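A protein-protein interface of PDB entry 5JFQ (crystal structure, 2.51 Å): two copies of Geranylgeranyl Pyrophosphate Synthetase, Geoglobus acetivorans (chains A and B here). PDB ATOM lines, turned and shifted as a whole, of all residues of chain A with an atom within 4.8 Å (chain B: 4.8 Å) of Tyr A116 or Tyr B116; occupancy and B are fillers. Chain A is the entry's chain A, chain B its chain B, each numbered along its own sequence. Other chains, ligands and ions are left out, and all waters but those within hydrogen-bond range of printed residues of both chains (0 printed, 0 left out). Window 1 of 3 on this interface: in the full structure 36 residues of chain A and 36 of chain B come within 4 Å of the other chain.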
ATOM      1  N   PHE A  79      29.536  35.261  15.422  1.00  0.00           N
ATOM      2  CA  PHE A  79      29.232  34.779  16.729  1.00  0.00           C
ATOM      3  C   PHE A  79      30.462  34.791  17.604  1.00  0.00           C
ATOM      4  O   PHE A  79      30.366  35.131  18.744  1.00  0.00           O
ATOM      5  CB  PHE A  79      28.574  33.401  16.672  1.00  0.00           C
ATOM      6  CG  PHE A  79      29.182  32.391  17.581  1.00  0.00           C
ATOM      7  CD1 PHE A  79      29.050  32.495  18.924  1.00  0.00           C
ATOM      8  CD2 PHE A  79      29.910  31.365  17.076  1.00  0.00           C
ATOM      9  CE1 PHE A  79      29.643  31.608  19.744  1.00  0.00           C
ATOM     10  CE2 PHE A  79      30.507  30.476  17.883  1.00  0.00           C
ATOM     11  CZ  PHE A  79      30.368  30.590  19.222  1.00  0.00           C
ATOM     12  N   GLY A 112      25.190  36.017  20.537  1.00  0.00           N
ATOM     13  CA  GLY A 112      26.109  35.060  19.954  1.00  0.00           C
ATOM     14  C   GLY A 112      25.465  33.700  19.807  1.00  0.00           C
ATOM     15  O   GLY A 112      25.523  33.093  18.735  1.00  0.00           O
ATOM     16  N   ASP A 113      24.803  33.233  20.876  1.00  0.00           N
ATOM     17  CA  ASP A 113      24.120  31.945  20.866  1.00  0.00           C
ATOM     18  C   ASP A 113      23.048  31.883  19.791  1.00  0.00           C
ATOM     19  O   ASP A 113      22.766  30.803  19.270  1.00  0.00           O
ATOM     20  CB  ASP A 113      23.486  31.662  22.232  1.00  0.00           C
ATOM     21  CG  ASP A 113      24.512  31.488  23.324  1.00  0.00           C
ATOM     22  OD1 ASP A 113      25.710  31.443  23.004  1.00  0.00           O
ATOM     23  OD2 ASP A 113      24.127  31.391  24.510  1.00  0.00           O
ATOM     24  N   THR A 114      22.416  33.012  19.471  1.00  0.00           N
ATOM     25  CA  THR A 114      21.433  33.015  18.399  1.00  0.00           C
ATOM     26  C   THR A 114      22.120  32.819  17.055  1.00  0.00           C
ATOM     27  O   THR A 114      21.767  31.914  16.282  1.00  0.00           O
ATOM     28  CB  THR A 114      20.634  34.325  18.404  1.00  0.00           C
ATOM     29  OG1 THR A 114      19.896  34.452  19.627  1.00  0.00           O
ATOM     30  CG2 THR A 114      19.664  34.368  17.213  1.00  0.00           C
ATOM     31  N   LEU A 115      23.110  33.669  16.764  1.00  0.00           N
ATOM     32  CA  LEU A 115      23.864  33.521  15.533  1.00  0.00           C
ATOM     33  C   LEU A 115      24.408  32.098  15.406  1.00  0.00           C
ATOM     34  O   LEU A 115      24.425  31.527  14.313  1.00  0.00           O
ATOM     35  CB  LEU A 115      24.991  34.545  15.510  1.00  0.00           C
ATOM     36  CG  LEU A 115      24.649  36.005  15.247  1.00  0.00           C
ATOM     37  CD1 LEU A 115      25.916  36.823  15.364  1.00  0.00           C
ATOM     38  CD2 LEU A 115      24.022  36.219  13.885  1.00  0.00           C
ATOM     39  N   TYR A 116      24.804  31.503  16.536  1.00  0.00           N
ATOM     40  CA  TYR A 116      25.407  30.179  16.547  1.00  0.00           C
ATOM     41  C   TYR A 116      24.454  29.145  15.975  1.00  0.00           C
ATOM     42  O   TYR A 116      24.825  28.363  15.091  1.00  0.00           O
ATOM     43  CB  TYR A 116      25.781  29.808  17.972  1.00  0.00           C
ATOM     44  CG  TYR A 116      26.981  28.900  18.158  1.00  0.00           C
ATOM     45  CD1 TYR A 116      27.579  28.824  19.398  1.00  0.00           C
ATOM     46  CD2 TYR A 116      27.502  28.097  17.124  1.00  0.00           C
ATOM     47  CE1 TYR A 116      28.664  28.013  19.636  1.00  0.00           C
ATOM     48  CE2 TYR A 116      28.613  27.268  17.350  1.00  0.00           C
ATOM     49  CZ  TYR A 116      29.193  27.253  18.633  1.00  0.00           C
ATOM     50  OH  TYR A 116      30.298  26.502  19.006  1.00  0.00           O
ATOM     51  N   ALA A 117      23.216  29.129  16.464  1.00  0.00           N
ATOM     52  CA  ALA A 117      22.264  28.146  15.970  1.00  0.00           C
ATOM     53  C   ALA A 117      21.891  28.434  14.527  1.00  0.00           C
ATOM     54  O   ALA A 117      21.772  27.506  13.719  1.00  0.00           O
ATOM     55  CB  ALA A 117      21.021  28.116  16.853  1.00  0.00           C
ATOM     56  N   GLU A 118      21.735  29.718  14.182  1.00  0.00           N
ATOM     57  CA  GLU A 118      21.355  30.083  12.823  1.00  0.00           C
ATOM     58  C   GLU A 118      22.390  29.592  11.827  1.00  0.00           C
ATOM     59  O   GLU A 118      22.035  29.056  10.770  1.00  0.00           O
ATOM     60  CB  GLU A 118      21.171  31.593  12.700  1.00  0.00           C
ATOM     61  CG  GLU A 118      20.050  32.118  13.564  1.00  0.00           C
ATOM     62  CD  GLU A 118      19.824  33.612  13.411  1.00  0.00           C
ATOM     63  OE1 GLU A 118      20.788  34.387  13.570  1.00  0.00           O
ATOM     64  OE2 GLU A 118      18.671  34.014  13.124  1.00  0.00           O
ATOM     65  N   ALA A 119      23.675  29.761  12.152  1.00  0.00           N
ATOM     66  CA  ALA A 119      24.740  29.219  11.324  1.00  0.00           C
ATOM     67  C   ALA A 119      24.387  27.808  10.888  1.00  0.00           C
ATOM     68  O   ALA A 119      24.314  27.515   9.694  1.00  0.00           O
ATOM     69  CB  ALA A 119      26.060  29.230  12.091  1.00  0.00           C
ATOM     70  N   PHE A 120      24.087  26.942  11.853  1.00  0.00           N
ATOM     71  CA  PHE A 120      23.788  25.567  11.502  1.00  0.00           C
ATOM     72  C   PHE A 120      22.482  25.471  10.740  1.00  0.00           C
ATOM     73  O   PHE A 120      22.377  24.695   9.783  1.00  0.00           O
ATOM     74  CB  PHE A 120      23.775  24.692  12.744  1.00  0.00           C
ATOM     75  CG  PHE A 120      25.136  24.434  13.284  1.00  0.00           C
ATOM     76  CD1 PHE A 120      25.931  23.429  12.738  1.00  0.00           C
ATOM     77  CD2 PHE A 120      25.650  25.212  14.308  1.00  0.00           C
ATOM     78  CE1 PHE A 120      27.221  23.195  13.229  1.00  0.00           C
ATOM     79  CE2 PHE A 120      26.935  24.985  14.804  1.00  0.00           C
ATOM     80  CZ  PHE A 120      27.721  23.984  14.267  1.00  0.00           C
ATOM     81  N   CYS A 144      34.101  24.724  15.273  1.00  0.00           N
ATOM     82  CA  CYS A 144      33.610  25.568  16.348  1.00  0.00           C
ATOM     83  C   CYS A 144      34.224  25.160  17.681  1.00  0.00           C
ATOM     84  O   CYS A 144      34.738  26.008  18.419  1.00  0.00           O
ATOM     85  CB  CYS A 144      32.085  25.517  16.388  1.00  0.00           C
ATOM     86  SG  CYS A 144      31.352  26.322  14.975  1.00  0.00           S
ATOM     87  N   CYS A 148      36.790  27.580  20.169  1.00  0.00           N
ATOM     88  CA  CYS A 148      36.675  27.760  21.607  1.00  0.00           C
ATOM     89  C   CYS A 148      37.942  27.314  22.316  1.00  0.00           C
ATOM     90  O   CYS A 148      38.414  27.981  23.246  1.00  0.00           O
ATOM     91  CB  CYS A 148      35.467  26.987  22.131  1.00  0.00           C
ATOM     92  SG  CYS A 148      33.924  27.510  21.370  1.00  0.00           S
ATOM     93  N   PHE B  79      24.314  23.183  27.659  1.00  0.00           N
ATOM     94  CA  PHE B  79      24.731  24.467  27.131  1.00  0.00           C
ATOM     95  C   PHE B  79      23.892  25.593  27.727  1.00  0.00           C
ATOM     96  O   PHE B  79      24.438  26.572  28.253  1.00  0.00           O
ATOM     97  CB  PHE B  79      24.636  24.446  25.603  1.00  0.00           C
ATOM     98  CG  PHE B  79      24.172  25.749  24.998  1.00  0.00           C
ATOM     99  CD1 PHE B  79      24.942  26.888  25.096  1.00  0.00           C
ATOM    100  CD2 PHE B  79      22.978  25.817  24.317  1.00  0.00           C
ATOM    101  CE1 PHE B  79      24.512  28.074  24.548  1.00  0.00           C
ATOM    102  CE2 PHE B  79      22.564  26.989  23.768  1.00  0.00           C
ATOM    103  CZ  PHE B  79      23.328  28.124  23.890  1.00  0.00           C
ATOM    104  N   GLY B 112      29.912  26.569  27.460  1.00  0.00           N
ATOM    105  CA  GLY B 112      28.644  26.386  26.774  1.00  0.00           C
ATOM    106  C   GLY B 112      28.782  26.458  25.263  1.00  0.00           C
ATOM    107  O   GLY B 112      28.140  25.694  24.538  1.00  0.00           O
ATOM    108  N   ASP B 113      29.625  27.376  24.765  1.00  0.00           N
ATOM    109  CA  ASP B 113      29.881  27.434  23.325  1.00  0.00           C
ATOM    110  C   ASP B 113      30.423  26.112  22.811  1.00  0.00           C
ATOM    111  O   ASP B 113      30.148  25.731  21.668  1.00  0.00           O
ATOM    112  CB  ASP B 113      30.873  28.542  22.991  1.00  0.00           C
ATOM    113  CG  ASP B 113      30.260  29.917  23.050  1.00  0.00           C
ATOM    114  OD1 ASP B 113      29.033  30.037  23.227  1.00  0.00           O
ATOM    115  OD2 ASP B 113      31.023  30.893  22.905  1.00  0.00           O
ATOM    116  N   THR B 114      31.196  25.410  23.647  1.00  0.00           N
ATOM    117  CA  THR B 114      31.763  24.121  23.279  1.00  0.00           C
ATOM    118  C   THR B 114      30.702  23.032  23.293  1.00  0.00           C
ATOM    119  O   THR B 114      30.562  22.269  22.330  1.00  0.00           O
ATOM    120  CB  THR B 114      32.890  23.748  24.236  1.00  0.00           C
ATOM    121  OG1 THR B 114      33.947  24.718  24.162  1.00  0.00           O
ATOM    122  CG2 THR B 114      33.417  22.357  23.883  1.00  0.00           C
ATOM    123  N   LEU B 115      29.957  22.932  24.390  1.00  0.00           N
ATOM    124  CA  LEU B 115      28.799  22.049  24.415  1.00  0.00           C
ATOM    125  C   LEU B 115      27.893  22.308  23.216  1.00  0.00           C
ATOM    126  O   LEU B 115      27.409  21.367  22.570  1.00  0.00           O
ATOM    127  CB  LEU B 115      28.041  22.237  25.734  1.00  0.00           C
ATOM    128  CG  LEU B 115      28.776  21.689  26.973  1.00  0.00           C
ATOM    129  CD1 LEU B 115      28.109  22.115  28.288  1.00  0.00           C
ATOM    130  CD2 LEU B 115      28.924  20.159  26.909  1.00  0.00           C
ATOM    131  N   TYR B 116      27.673  23.585  22.894  1.00  0.00           N
ATOM    132  CA  TYR B 116      26.772  23.956  21.803  1.00  0.00           C
ATOM    133  C   TYR B 116      27.216  23.323  20.489  1.00  0.00           C
ATOM    134  O   TYR B 116      26.416  22.704  19.788  1.00  0.00           O
ATOM    135  CB  TYR B 116      26.735  25.481  21.684  1.00  0.00           C
ATOM    136  CG  TYR B 116      25.471  26.151  21.150  1.00  0.00           C
ATOM    137  CD1 TYR B 116      24.425  25.438  20.547  1.00  0.00           C
ATOM    138  CD2 TYR B 116      25.353  27.535  21.246  1.00  0.00           C
ATOM    139  CE1 TYR B 116      23.289  26.116  20.060  1.00  0.00           C
ATOM    140  CE2 TYR B 116      24.254  28.218  20.769  1.00  0.00           C
ATOM    141  CZ  TYR B 116      23.222  27.527  20.189  1.00  0.00           C
ATOM    142  OH  TYR B 116      22.158  28.302  19.760  1.00  0.00           O
ATOM    143  N   ALA B 117      28.492  23.485  20.129  1.00  0.00           N
ATOM    144  CA  ALA B 117      28.995  22.843  18.921  1.00  0.00           C
ATOM    145  C   ALA B 117      28.992  21.325  19.075  1.00  0.00           C
ATOM    146  O   ALA B 117      28.617  20.596  18.142  1.00  0.00           O
ATOM    147  CB  ALA B 117      30.404  23.349  18.587  1.00  0.00           C
ATOM    148  N   GLU B 118      29.388  20.833  20.255  1.00  0.00           N
ATOM    149  CA  GLU B 118      29.476  19.395  20.444  1.00  0.00           C
ATOM    150  C   GLU B 118      28.135  18.730  20.185  1.00  0.00           C
ATOM    151  O   GLU B 118      28.090  17.617  19.640  1.00  0.00           O
ATOM    152  CB  GLU B 118      30.002  19.076  21.841  1.00  0.00           C
ATOM    153  CG  GLU B 118      31.523  19.098  21.931  1.00  0.00           C
ATOM    154  CD  GLU B 118      32.058  18.885  23.353  1.00  0.00           C
ATOM    155  OE1 GLU B 118      31.427  19.375  24.331  1.00  0.00           O
ATOM    156  OE2 GLU B 118      33.129  18.234  23.487  1.00  0.00           O
ATOM    157  N   ALA B 119      27.039  19.431  20.487  1.00  0.00           N
ATOM    158  CA  ALA B 119      25.712  18.853  20.293  1.00  0.00           C
ATOM    159  C   ALA B 119      25.422  18.629  18.819  1.00  0.00           C
ATOM    160  O   ALA B 119      24.857  17.598  18.438  1.00  0.00           O
ATOM    161  CB  ALA B 119      24.636  19.746  20.911  1.00  0.00           C
ATOM    162  N   PHE B 120      25.773  19.592  17.976  1.00  0.00           N
ATOM    163  CA  PHE B 120      25.551  19.387  16.558  1.00  0.00           C
ATOM    164  C   PHE B 120      26.500  18.338  15.988  1.00  0.00           C
ATOM    165  O   PHE B 120      26.142  17.644  15.032  1.00  0.00           O
ATOM    166  CB  PHE B 120      25.660  20.713  15.830  1.00  0.00           C
ATOM    167  CG  PHE B 120      24.466  21.573  16.027  1.00  0.00           C
ATOM    168  CD1 PHE B 120      23.305  21.336  15.303  1.00  0.00           C
ATOM    169  CD2 PHE B 120      24.470  22.574  16.985  1.00  0.00           C
ATOM    170  CE1 PHE B 120      22.190  22.106  15.493  1.00  0.00           C
ATOM    171  CE2 PHE B 120      23.342  23.362  17.191  1.00  0.00           C
ATOM    172  CZ  PHE B 120      22.200  23.137  16.446  1.00  0.00           C
ATOM    173  N   CYS B 144      17.081  25.965  19.129  1.00  0.00           N
ATOM    174  CA  CYS B 144      18.083  26.718  19.871  1.00  0.00           C
ATOM    175  C   CYS B 144      17.893  28.221  19.692  1.00  0.00           C
ATOM    176  O   CYS B 144      18.084  28.995  20.634  1.00  0.00           O
ATOM    177  CB  CYS B 144      19.478  26.280  19.433  1.00  0.00           C
ATOM    178  SG  CYS B 144      19.894  24.579  19.925  1.00  0.00           S
ATOM    179  N   CYS B 148      16.938  30.894  22.893  1.00  0.00           N
ATOM    180  CA  CYS B 148      17.568  32.201  23.045  1.00  0.00           C
ATOM    181  C   CYS B 148      16.522  33.307  23.012  1.00  0.00           C
ATOM    182  O   CYS B 148      16.567  34.251  23.810  1.00  0.00           O
ATOM    183  CB  CYS B 148      18.605  32.421  21.940  1.00  0.00           C
ATOM    184  SG  CYS B 148      19.980  31.265  21.934  1.00  0.00           S
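O of Asp A113 lies within hydrogen-bond range of OH of Tyr B116, at 2.6 Å.
O of Asp B113 lies within hydrogen-bond range of OH of Tyr A116.
The backbone carbonyl oxygen of Cys A144 is in hydrogen-bond range of the side-chain sulfur of Cys A148, at 3.4 Å.
O of Cys B144 sits at hydrogen-bond distance from SG of Cys B148 (3.2 Å).
Phe A79 touches Asp B113.
Asp A113 touches Phe B79 (OD2 to CE1, 3.3 Å).
OD1 of Asp A113 touches OD1 of Asp B113, 3.6 Å away.
Cys B148 touches Asp A113.
CB of Cys B148 touches OG1 of Thr A114, at 3.3 Å.
Tyr A116 touches Ala B117.
Ala A117 touches Tyr B116.
Cys B144 touches Ala A117 (CB to CB, 3.5 Å).
Phe A120 touches Phe B120.
SG of Cys A148 touches CB of Asp B113, 3.6 Å away.
Tyr A116 touches just these residues of chain B: Asp B113, Tyr B116 and Ala B117.
Tyr B116 touches just these residues of chain A: Asp A113, Tyr A116 and Ala A117.
Printed residues of chain B within 4 Å of Cys A144: Ala B117 (3.5 Å).
Printed residues of chain B within 4 Å of Phe A79: Asp B113 (3.5 Å).
Of the printed residues of chain B, Thr A114 touches Cys B148.
Of the printed residues of chain B, Asp A113 touches Phe B79, Asp B113, Tyr B116 and Cys B148.
Gly A112 touches none of the printed residues of chain B.
Glu B118 touches none of the printed residues of chain A.
The nearest printed residue of chain B that does not touch Tyr A116 is Thr B114 (4.9 Å).
The nearest residue of chain A that does not touch Tyr B116 is Thr A114 (4.7 Å).
Of the 12 printed residues of chain B, 8 touch a printed residue of chain A.
Hydrophobic or aromatic side chains of chain B that line the printed part of chain A: Phe B79, Tyr B116, Ala B117 and Phe B120.
Along chain B the printed residues that touch a printed residue of chain A span positions 79 to 148.
Of the 12 printed residues of chain A, 8 touch a printed residue of chain B.
Printed residues of chain A that touch a printed residue of chain B: Phe A79, Asp A113, Thr A114, Tyr A116, Ala A117, Phe A120, Cys A144 and Cys A148.
Among the printed residues, 15 pairs touch across the chains.
Among the printed residues, no Asp or Glu carboxylate lies within 4 Å of a Lys or Arg side-chain nitrogen of the other chain.
Phe A79 touches Asp B113, and with the chains exchanged Asp A113 touches Phe B79.
Asp A113 touches Tyr B116, and with the chains exchanged Tyr A116 touches Asp B113.
Thr A114 touches Cys B148, and with the chains exchanged Cys A148 touches Thr B114.
Phe B120 touches its own counterpart, Phe A120.
Of the 15 pairs that touch across the chains among the printed residues, 15 have their exchanged pair printed and touching as well.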
